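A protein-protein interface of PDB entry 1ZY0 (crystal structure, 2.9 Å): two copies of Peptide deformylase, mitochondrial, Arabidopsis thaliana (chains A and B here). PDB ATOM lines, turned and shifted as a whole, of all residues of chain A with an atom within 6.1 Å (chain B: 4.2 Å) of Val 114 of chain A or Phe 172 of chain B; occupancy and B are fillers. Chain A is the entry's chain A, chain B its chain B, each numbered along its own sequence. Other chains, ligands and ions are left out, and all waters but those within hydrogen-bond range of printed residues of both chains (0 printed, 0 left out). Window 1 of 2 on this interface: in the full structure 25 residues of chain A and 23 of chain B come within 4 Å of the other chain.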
ATOM      1  N   VAL A   7     -15.671  -0.906  -7.345  1.00  0.00           N
ATOM      2  CA  VAL A   7     -16.361  -2.161  -7.618  1.00  0.00           C
ATOM      3  C   VAL A   7     -15.351  -3.283  -7.773  1.00  0.00           C
ATOM      4  O   VAL A   7     -14.245  -3.065  -8.249  1.00  0.00           O
ATOM      5  CB  VAL A   7     -17.198  -2.072  -8.884  1.00  0.00           C
ATOM      6  CG1 VAL A   7     -18.445  -1.268  -8.622  1.00  0.00           C
ATOM      7  CG2 VAL A   7     -16.398  -1.419  -9.970  1.00  0.00           C
ATOM      8  N   ALA A   8     -15.741  -4.484  -7.369  1.00  0.00           N
ATOM      9  CA  ALA A   8     -14.857  -5.639  -7.440  1.00  0.00           C
ATOM     10  C   ALA A   8     -15.246  -6.575  -8.574  1.00  0.00           C
ATOM     11  O   ALA A   8     -16.347  -6.494  -9.113  1.00  0.00           O
ATOM     12  CB  ALA A   8     -14.871  -6.390  -6.115  1.00  0.00           C
ATOM     13  N   SER A   9     -14.334  -7.470  -8.929  1.00  0.00           N
ATOM     14  CA  SER A   9     -14.597  -8.400 -10.001  1.00  0.00           C
ATOM     15  C   SER A   9     -15.985  -8.998  -9.874  1.00  0.00           C
ATOM     16  O   SER A   9     -16.540  -9.089  -8.789  1.00  0.00           O
ATOM     17  CB  SER A   9     -13.541  -9.488 -10.008  1.00  0.00           C
ATOM     18  OG  SER A   9     -12.267  -8.916 -10.250  1.00  0.00           O
ATOM     19  N   GLY A  10     -16.538  -9.407 -11.005  1.00  0.00           N
ATOM     20  CA  GLY A  10     -17.869  -9.961 -11.004  1.00  0.00           C
ATOM     21  C   GLY A  10     -18.801  -8.905 -11.537  1.00  0.00           C
ATOM     22  O   GLY A  10     -19.634  -9.168 -12.387  1.00  0.00           O
ATOM     23  N   HIS A  15     -15.938  -5.774 -16.559  1.00  0.00           N
ATOM     24  CA  HIS A  15     -15.596  -6.659 -17.657  1.00  0.00           C
ATOM     25  C   HIS A  15     -16.350  -6.383 -18.946  1.00  0.00           C
ATOM     26  O   HIS A  15     -16.747  -7.308 -19.658  1.00  0.00           O
ATOM     27  CB  HIS A  15     -15.814  -8.108 -17.239  1.00  0.00           C
ATOM     28  CG  HIS A  15     -15.527  -8.368 -15.789  1.00  0.00           C
ATOM     29  ND1 HIS A  15     -16.509  -8.338 -14.817  1.00  0.00           N
ATOM     30  CD2 HIS A  15     -14.371  -8.657 -15.141  1.00  0.00           C
ATOM     31  CE1 HIS A  15     -15.971  -8.601 -13.642  1.00  0.00           C
ATOM     32  NE2 HIS A  15     -14.675  -8.799 -13.809  1.00  0.00           N
ATOM     33  N   GLY A 110      -1.418  -5.436  -9.052  1.00  0.00           N
ATOM     34  CA  GLY A 110      -2.559  -5.625  -8.195  1.00  0.00           C
ATOM     35  C   GLY A 110      -3.600  -4.694  -8.754  1.00  0.00           C
ATOM     36  O   GLY A 110      -3.307  -3.876  -9.639  1.00  0.00           O
ATOM     37  N   CYS A 111      -4.812  -4.802  -8.265  1.00  0.00           N
ATOM     38  CA  CYS A 111      -5.874  -3.951  -8.727  1.00  0.00           C
ATOM     39  C   CYS A 111      -6.776  -3.764  -7.536  1.00  0.00           C
ATOM     40  O   CYS A 111      -6.969  -4.692  -6.745  1.00  0.00           O
ATOM     41  CB  CYS A 111      -6.621  -4.615  -9.860  1.00  0.00           C
ATOM     42  SG  CYS A 111      -8.068  -3.714 -10.287  1.00  0.00           S
ATOM     43  N   LEU A 112      -7.336  -2.573  -7.388  1.00  0.00           N
ATOM     44  CA  LEU A 112      -8.179  -2.350  -6.234  1.00  0.00           C
ATOM     45  C   LEU A 112      -9.496  -3.084  -6.322  1.00  0.00           C
ATOM     46  O   LEU A 112     -10.241  -3.130  -5.375  1.00  0.00           O
ATOM     47  CB  LEU A 112      -8.404  -0.869  -6.035  1.00  0.00           C
ATOM     48  CG  LEU A 112      -7.049  -0.202  -5.806  1.00  0.00           C
ATOM     49  CD1 LEU A 112      -6.483   0.259  -7.107  1.00  0.00           C
ATOM     50  CD2 LEU A 112      -7.196   0.948  -4.885  1.00  0.00           C
ATOM     51  N   SER A 113      -9.751  -3.683  -7.484  1.00  0.00           N
ATOM     52  CA  SER A 113     -10.982  -4.438  -7.671  1.00  0.00           C
ATOM     53  C   SER A 113     -10.732  -5.907  -7.335  1.00  0.00           C
ATOM     54  O   SER A 113     -11.640  -6.740  -7.378  1.00  0.00           O
ATOM     55  CB  SER A 113     -11.456  -4.300  -9.117  1.00  0.00           C
ATOM     56  OG  SER A 113     -11.800  -2.962  -9.423  1.00  0.00           O
ATOM     57  N   VAL A 114      -9.489  -6.208  -6.983  1.00  0.00           N
ATOM     58  CA  VAL A 114      -9.068  -7.557  -6.637  1.00  0.00           C
ATOM     59  C   VAL A 114      -7.982  -7.411  -5.602  1.00  0.00           C
ATOM     60  O   VAL A 114      -6.793  -7.509  -5.930  1.00  0.00           O
ATOM     61  CB  VAL A 114      -8.468  -8.288  -7.860  1.00  0.00           C
ATOM     62  CG1 VAL A 114      -7.806  -9.590  -7.430  1.00  0.00           C
ATOM     63  CG2 VAL A 114      -9.556  -8.559  -8.877  1.00  0.00           C
ATOM     64  N   ASP A 115      -8.368  -7.173  -4.354  1.00  0.00           N
ATOM     65  CA  ASP A 115      -7.344  -6.991  -3.333  1.00  0.00           C
ATOM     66  C   ASP A 115      -7.053  -8.260  -2.558  1.00  0.00           C
ATOM     67  O   ASP A 115      -7.890  -9.152  -2.457  1.00  0.00           O
ATOM     68  CB  ASP A 115      -7.713  -5.846  -2.375  1.00  0.00           C
ATOM     69  CG  ASP A 115      -8.589  -6.295  -1.233  1.00  0.00           C
ATOM     70  OD1 ASP A 115      -9.656  -6.882  -1.497  1.00  0.00           O
ATOM     71  OD2 ASP A 115      -8.206  -6.055  -0.069  1.00  0.00           O
ATOM     72  N   GLY A 116      -5.843  -8.321  -2.019  1.00  0.00           N
ATOM     73  CA  GLY A 116      -5.419  -9.481  -1.267  1.00  0.00           C
ATOM     74  C   GLY A 116      -4.604 -10.325  -2.210  1.00  0.00           C
ATOM     75  O   GLY A 116      -3.945 -11.283  -1.808  1.00  0.00           O
ATOM     76  N   PHE A 117      -4.628  -9.944  -3.480  1.00  0.00           N
ATOM     77  CA  PHE A 117      -3.898 -10.699  -4.475  1.00  0.00           C
ATOM     78  C   PHE A 117      -2.998  -9.926  -5.413  1.00  0.00           C
ATOM     79  O   PHE A 117      -3.235  -8.768  -5.734  1.00  0.00           O
ATOM     80  CB  PHE A 117      -4.877 -11.549  -5.273  1.00  0.00           C
ATOM     81  CG  PHE A 117      -5.472 -12.655  -4.477  1.00  0.00           C
ATOM     82  CD1 PHE A 117      -4.818 -13.876  -4.365  1.00  0.00           C
ATOM     83  CD2 PHE A 117      -6.660 -12.464  -3.793  1.00  0.00           C
ATOM     84  CE1 PHE A 117      -5.337 -14.893  -3.583  1.00  0.00           C
ATOM     85  CE2 PHE A 117      -7.192 -13.470  -3.003  1.00  0.00           C
ATOM     86  CZ  PHE A 117      -6.531 -14.693  -2.900  1.00  0.00           C
ATOM     87  N   ARG A 118      -1.964 -10.620  -5.850  1.00  0.00           N
ATOM     88  CA  ARG A 118      -0.969 -10.084  -6.734  1.00  0.00           C
ATOM     89  C   ARG A 118      -0.602 -11.169  -7.724  1.00  0.00           C
ATOM     90  O   ARG A 118      -0.736 -12.360  -7.440  1.00  0.00           O
ATOM     91  CB  ARG A 118       0.268  -9.694  -5.927  1.00  0.00           C
ATOM     92  CG  ARG A 118       0.031  -8.591  -4.935  1.00  0.00           C
ATOM     93  CD  ARG A 118      -0.397  -7.342  -5.689  1.00  0.00           C
ATOM     94  NE  ARG A 118      -0.476  -6.161  -4.841  1.00  0.00           N
ATOM     95  CZ  ARG A 118      -1.421  -5.922  -3.951  1.00  0.00           C
ATOM     96  NH1 ARG A 118      -2.385  -6.769  -3.826  1.00  0.00           N
ATOM     97  NH2 ARG A 118      -1.427  -4.843  -3.225  1.00  0.00           N
ATOM     98  N   LEU A 162      -8.940  -7.485 -17.025  1.00  0.00           N
ATOM     99  CA  LEU A 162      -8.286  -7.384 -15.724  1.00  0.00           C
ATOM    100  C   LEU A 162      -6.997  -8.184 -15.782  1.00  0.00           C
ATOM    101  O   LEU A 162      -6.904  -9.135 -16.547  1.00  0.00           O
ATOM    102  CB  LEU A 162      -9.204  -7.907 -14.625  1.00  0.00           C
ATOM    103  CG  LEU A 162     -10.203  -6.857 -14.141  1.00  0.00           C
ATOM    104  CD1 LEU A 162     -11.018  -7.363 -12.973  1.00  0.00           C
ATOM    105  CD2 LEU A 162      -9.419  -5.632 -13.715  1.00  0.00           C
ATOM    106  N   TYR A 163      -6.003  -7.816 -14.982  1.00  0.00           N
ATOM    107  CA  TYR A 163      -4.729  -8.521 -15.059  1.00  0.00           C
ATOM    108  C   TYR A 163      -4.800 -10.039 -14.938  1.00  0.00           C
ATOM    109  O   TYR A 163      -4.062 -10.747 -15.623  1.00  0.00           O
ATOM    110  CB  TYR A 163      -3.733  -7.944 -14.046  1.00  0.00           C
ATOM    111  CG  TYR A 163      -3.928  -8.345 -12.604  1.00  0.00           C
ATOM    112  CD1 TYR A 163      -3.298  -9.467 -12.078  1.00  0.00           C
ATOM    113  CD2 TYR A 163      -4.685  -7.562 -11.746  1.00  0.00           C
ATOM    114  CE1 TYR A 163      -3.414  -9.791 -10.727  1.00  0.00           C
ATOM    115  CE2 TYR A 163      -4.808  -7.877 -10.398  1.00  0.00           C
ATOM    116  CZ  TYR A 163      -4.171  -8.989  -9.892  1.00  0.00           C
ATOM    117  OH  TYR A 163      -4.286  -9.273  -8.552  1.00  0.00           O
ATOM    118  N   VAL A 164      -5.699 -10.537 -14.099  1.00  0.00           N
ATOM    119  CA  VAL A 164      -5.836 -11.973 -13.895  1.00  0.00           C
ATOM    120  C   VAL A 164      -5.919 -12.800 -15.180  1.00  0.00           C
ATOM    121  O   VAL A 164      -5.496 -13.958 -15.206  1.00  0.00           O
ATOM    122  CB  VAL A 164      -7.058 -12.284 -13.024  1.00  0.00           C
ATOM    123  CG1 VAL A 164      -6.911 -11.605 -11.675  1.00  0.00           C
ATOM    124  CG2 VAL A 164      -8.324 -11.841 -13.731  1.00  0.00           C
ATOM    125  N   ASP A 165      -6.462 -12.218 -16.241  1.00  0.00           N
ATOM    126  CA  ASP A 165      -6.567 -12.929 -17.504  1.00  0.00           C
ATOM    127  C   ASP A 165      -5.365 -12.571 -18.383  1.00  0.00           C
ATOM    128  O   ASP A 165      -5.422 -12.677 -19.600  1.00  0.00           O
ATOM    129  CB  ASP A 165      -7.876 -12.560 -18.226  1.00  0.00           C
ATOM    130  CG  ASP A 165      -9.121 -12.739 -17.351  1.00  0.00           C
ATOM    131  OD1 ASP A 165      -9.438 -13.873 -16.938  1.00  0.00           O
ATOM    132  OD2 ASP A 165      -9.795 -11.727 -17.084  1.00  0.00           O
ATOM    133  N   PHE A 172       0.236 -15.996  -9.508  1.00  0.00           N
ATOM    134  CA  PHE A 172      -0.885 -15.413  -8.782  1.00  0.00           C
ATOM    135  C   PHE A 172      -0.638 -15.721  -7.319  1.00  0.00           C
ATOM    136  O   PHE A 172      -0.159 -16.806  -6.992  1.00  0.00           O
ATOM    137  CB  PHE A 172      -2.183 -16.069  -9.257  1.00  0.00           C
ATOM    138  CG  PHE A 172      -3.410 -15.496  -8.633  1.00  0.00           C
ATOM    139  CD1 PHE A 172      -4.151 -16.230  -7.725  1.00  0.00           C
ATOM    140  CD2 PHE A 172      -3.864 -14.240  -8.998  1.00  0.00           C
ATOM    141  CE1 PHE A 172      -5.309 -15.701  -7.145  1.00  0.00           C
ATOM    142  CE2 PHE A 172      -5.019 -13.697  -8.425  1.00  0.00           C
ATOM    143  CZ  PHE A 172      -5.755 -14.441  -7.514  1.00  0.00           C
ATOM    144  N   PHE B 117     -12.823 -15.499  -3.680  1.00  0.00           N
ATOM    145  CA  PHE B 117     -12.961 -15.476  -5.119  1.00  0.00           C
ATOM    146  C   PHE B 117     -13.473 -16.732  -5.767  1.00  0.00           C
ATOM    147  O   PHE B 117     -13.269 -17.843  -5.279  1.00  0.00           O
ATOM    148  CB  PHE B 117     -11.642 -15.082  -5.744  1.00  0.00           C
ATOM    149  CG  PHE B 117     -11.285 -13.652  -5.503  1.00  0.00           C
ATOM    150  CD1 PHE B 117     -11.754 -12.658  -6.349  1.00  0.00           C
ATOM    151  CD2 PHE B 117     -10.517 -13.290  -4.403  1.00  0.00           C
ATOM    152  CE1 PHE B 117     -11.459 -11.320  -6.097  1.00  0.00           C
ATOM    153  CE2 PHE B 117     -10.219 -11.957  -4.144  1.00  0.00           C
ATOM    154  CZ  PHE B 117     -10.691 -10.972  -4.990  1.00  0.00           C
ATOM    155  N   ARG B 118     -14.138 -16.518  -6.893  1.00  0.00           N
ATOM    156  CA  ARG B 118     -14.731 -17.579  -7.676  1.00  0.00           C
ATOM    157  C   ARG B 118     -14.497 -17.266  -9.139  1.00  0.00           C
ATOM    158  O   ARG B 118     -14.340 -16.111  -9.516  1.00  0.00           O
ATOM    159  CB  ARG B 118     -16.230 -17.624  -7.411  1.00  0.00           C
ATOM    160  CG  ARG B 118     -16.581 -17.927  -5.975  1.00  0.00           C
ATOM    161  CD  ARG B 118     -16.191 -19.489  -5.676  1.00  0.00           C
ATOM    162  NE  ARG B 118     -16.773 -19.617  -4.321  1.00  0.00           N
ATOM    163  CZ  ARG B 118     -16.011 -19.580  -3.252  1.00  0.00           C
ATOM    164  NH1 ARG B 118     -14.723 -19.709  -3.302  1.00  0.00           N
ATOM    165  NH2 ARG B 118     -16.607 -19.850  -2.070  1.00  0.00           N
ATOM    166  N   ALA B 119     -14.475 -18.302  -9.965  1.00  0.00           N
ATOM    167  CA  ALA B 119     -14.285 -18.101 -11.388  1.00  0.00           C
ATOM    168  C   ALA B 119     -14.878 -19.268 -12.139  1.00  0.00           C
ATOM    169  O   ALA B 119     -14.849 -20.404 -11.675  1.00  0.00           O
ATOM    170  CB  ALA B 119     -12.813 -17.956 -11.716  1.00  0.00           C
ATOM    171  N   MET B 167      -9.461 -20.366 -15.754  1.00  0.00           N
ATOM    172  CA  MET B 167     -10.762 -19.732 -15.778  1.00  0.00           C
ATOM    173  C   MET B 167     -11.057 -19.048 -17.100  1.00  0.00           C
ATOM    174  O   MET B 167     -10.182 -18.641 -17.823  1.00  0.00           O
ATOM    175  CB  MET B 167     -10.868 -18.740 -14.624  1.00  0.00           C
ATOM    176  CG  MET B 167      -9.679 -17.813 -14.506  1.00  0.00           C
ATOM    177  SD  MET B 167      -9.734 -16.860 -13.000  1.00  0.00           S
ATOM    178  CE  MET B 167      -8.968 -15.346 -13.536  1.00  0.00           C
ATOM    179  N   ARG B 170     -12.594 -13.096 -17.765  1.00  0.00           N
ATOM    180  CA  ARG B 170     -13.561 -12.145 -17.222  1.00  0.00           C
ATOM    181  C   ARG B 170     -14.777 -12.746 -16.539  1.00  0.00           C
ATOM    182  O   ARG B 170     -15.886 -12.282 -16.762  1.00  0.00           O
ATOM    183  CB  ARG B 170     -14.021 -11.166 -18.279  1.00  0.00           C
ATOM    184  CG  ARG B 170     -13.092 -10.947 -19.427  1.00  0.00           C
ATOM    185  CD  ARG B 170     -13.328  -9.681 -20.339  1.00  0.00           C
ATOM    186  NE  ARG B 170     -13.250 -10.201 -21.758  1.00  0.00           N
ATOM    187  CZ  ARG B 170     -13.228  -9.291 -22.826  1.00  0.00           C
ATOM    188  NH1 ARG B 170     -14.071  -8.266 -22.796  1.00  0.00           N
ATOM    189  NH2 ARG B 170     -13.502 -10.017 -23.854  1.00  0.00           N
ATOM    190  N   THR B 171     -14.577 -13.781 -15.734  1.00  0.00           N
ATOM    191  CA  THR B 171     -15.676 -14.405 -15.013  1.00  0.00           C
ATOM    192  C   THR B 171     -15.212 -14.415 -13.569  1.00  0.00           C
ATOM    193  O   THR B 171     -16.000 -14.576 -12.642  1.00  0.00           O
ATOM    194  CB  THR B 171     -15.949 -15.845 -15.500  1.00  0.00           C
ATOM    195  OG1 THR B 171     -14.821 -16.679 -15.220  1.00  0.00           O
ATOM    196  CG2 THR B 171     -16.198 -15.853 -16.985  1.00  0.00           C
ATOM    197  N   PHE B 172     -13.905 -14.234 -13.405  1.00  0.00           N
ATOM    198  CA  PHE B 172     -13.270 -14.182 -12.098  1.00  0.00           C
ATOM    199  C   PHE B 172     -14.063 -13.175 -11.289  1.00  0.00           C
ATOM    200  O   PHE B 172     -14.497 -12.168 -11.830  1.00  0.00           O
ATOM    201  CB  PHE B 172     -11.820 -13.723 -12.256  1.00  0.00           C
ATOM    202  CG  PHE B 172     -11.029 -13.715 -10.976  1.00  0.00           C
ATOM    203  CD1 PHE B 172     -10.674 -12.521 -10.373  1.00  0.00           C
ATOM    204  CD2 PHE B 172     -10.629 -14.906 -10.372  1.00  0.00           C
ATOM    205  CE1 PHE B 172      -9.924 -12.508  -9.202  1.00  0.00           C
ATOM    206  CE2 PHE B 172      -9.882 -14.899  -9.201  1.00  0.00           C
ATOM    207  CZ  PHE B 172      -9.533 -13.695  -8.616  1.00  0.00           C
ATOM    208  N   ARG B 173     -14.263 -13.442 -10.003  1.00  0.00           N
ATOM    209  CA  ARG B 173     -15.045 -12.529  -9.189  1.00  0.00           C
ATOM    210  C   ARG B 173     -15.002 -12.765  -7.703  1.00  0.00           C
ATOM    211  O   ARG B 173     -14.489 -13.772  -7.212  1.00  0.00           O
ATOM    212  CB  ARG B 173     -16.501 -12.578  -9.618  1.00  0.00           C
ATOM    213  CG  ARG B 173     -17.139 -13.925  -9.367  1.00  0.00           C
ATOM    214  CD  ARG B 173     -18.455 -14.019 -10.090  1.00  0.00           C
ATOM    215  NE  ARG B 173     -18.288 -13.677 -11.497  1.00  0.00           N
ATOM    216  CZ  ARG B 173     -19.279 -13.311 -12.300  1.00  0.00           C
ATOM    217  NH1 ARG B 173     -20.513 -13.241 -11.834  1.00  0.00           N
ATOM    218  NH2 ARG B 173     -19.033 -12.988 -13.561  1.00  0.00           N
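Phe 117 of chain B touches its own counterpart, Phe 117 of chain A.
Val 114 of chain A touches one residue of chain B.
Printed residues of chain A within 4 Å of Phe 172 of chain B: Ser 9 (3.4 Å), Gly 10 (3.5 Å), His 15 (3.9 Å) and Val 114 (3.98 Å).
Printed residues of chain A within 4 Å of Phe 117 of chain B: Phe 117.
Of the printed residues of chain B, Phe 117 of chain A touches Phe 117.
Leu 162 of chain A touches none of the printed residues of chain B.
Ala 8 of chain A touches none of the printed residues of chain B.
Among the printed residues, pairs that only touch across the chains: Ser 9 of chain A with Phe 172 of chain B (3.4 Å), Ser 9 of chain A with Arg 173 of chain B (3.5 Å), Gly 10 of chain A with Phe 172 of chain B (3.5 Å), Gly 10 of chain A with Arg 173 of chain B (3.3 Å), His 15 of chain A with Arg 170 of chain B (3.7 Å), His 15 of chain A with Phe 172 of chain B (3.9 Å), Val 114 of chain A with Phe 172 of chain B (3.98 Å), Phe 117 of chain A with Phe 117 of chain B (3.6 Å), Val 164 of chain A with Met 167 of chain B (3.6 Å) and Asp 165 of chain A with Met 167 of chain B (3.7 Å).
The side-chain carboxylate of Asp 165 of chain A is in hydrogen-bond range of the backbone NH of Arg 170 of chain B (3.2 Å).
Of the 8 printed residues of chain B, 5 touch a printed residue of chain A.
Hydrophobic or aromatic side chains of chain B that line the printed part of chain A: Phe 117, Met 167 and Phe 172.
Printed residues of chain A that touch a printed residue of chain B: Ser 9, Gly 10, His 15, Val 114, Phe 117, Val 164 and Asp 165.
Among the printed residues, 11 pairs touch across the chains.
Among the printed residues, no Asp or Glu carboxylate lies within 4 Å of a Lys or Arg side-chain nitrogen of the other chain.
O of Ser 113 of chain A is in hydrogen-bond range of N of Ser 9 of chain A, 3.2 Å away.
N of Gly 10 of chain A lies close to NE2 of His 15 of chain A.
OH of Tyr 163 of chain A lies within hydrogen-bond range of O of Phe 117 of chain A, at 3.0 Å.
The backbone carbonyl oxygen of Arg 118 of chain B lies within hydrogen-bond range of the backbone NH of Arg 173 of chain B (2.7 Å).
O of Thr 171 of chain B sits at hydrogen-bond distance from NE of Arg 173 of chain B, at 2.7 Å.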
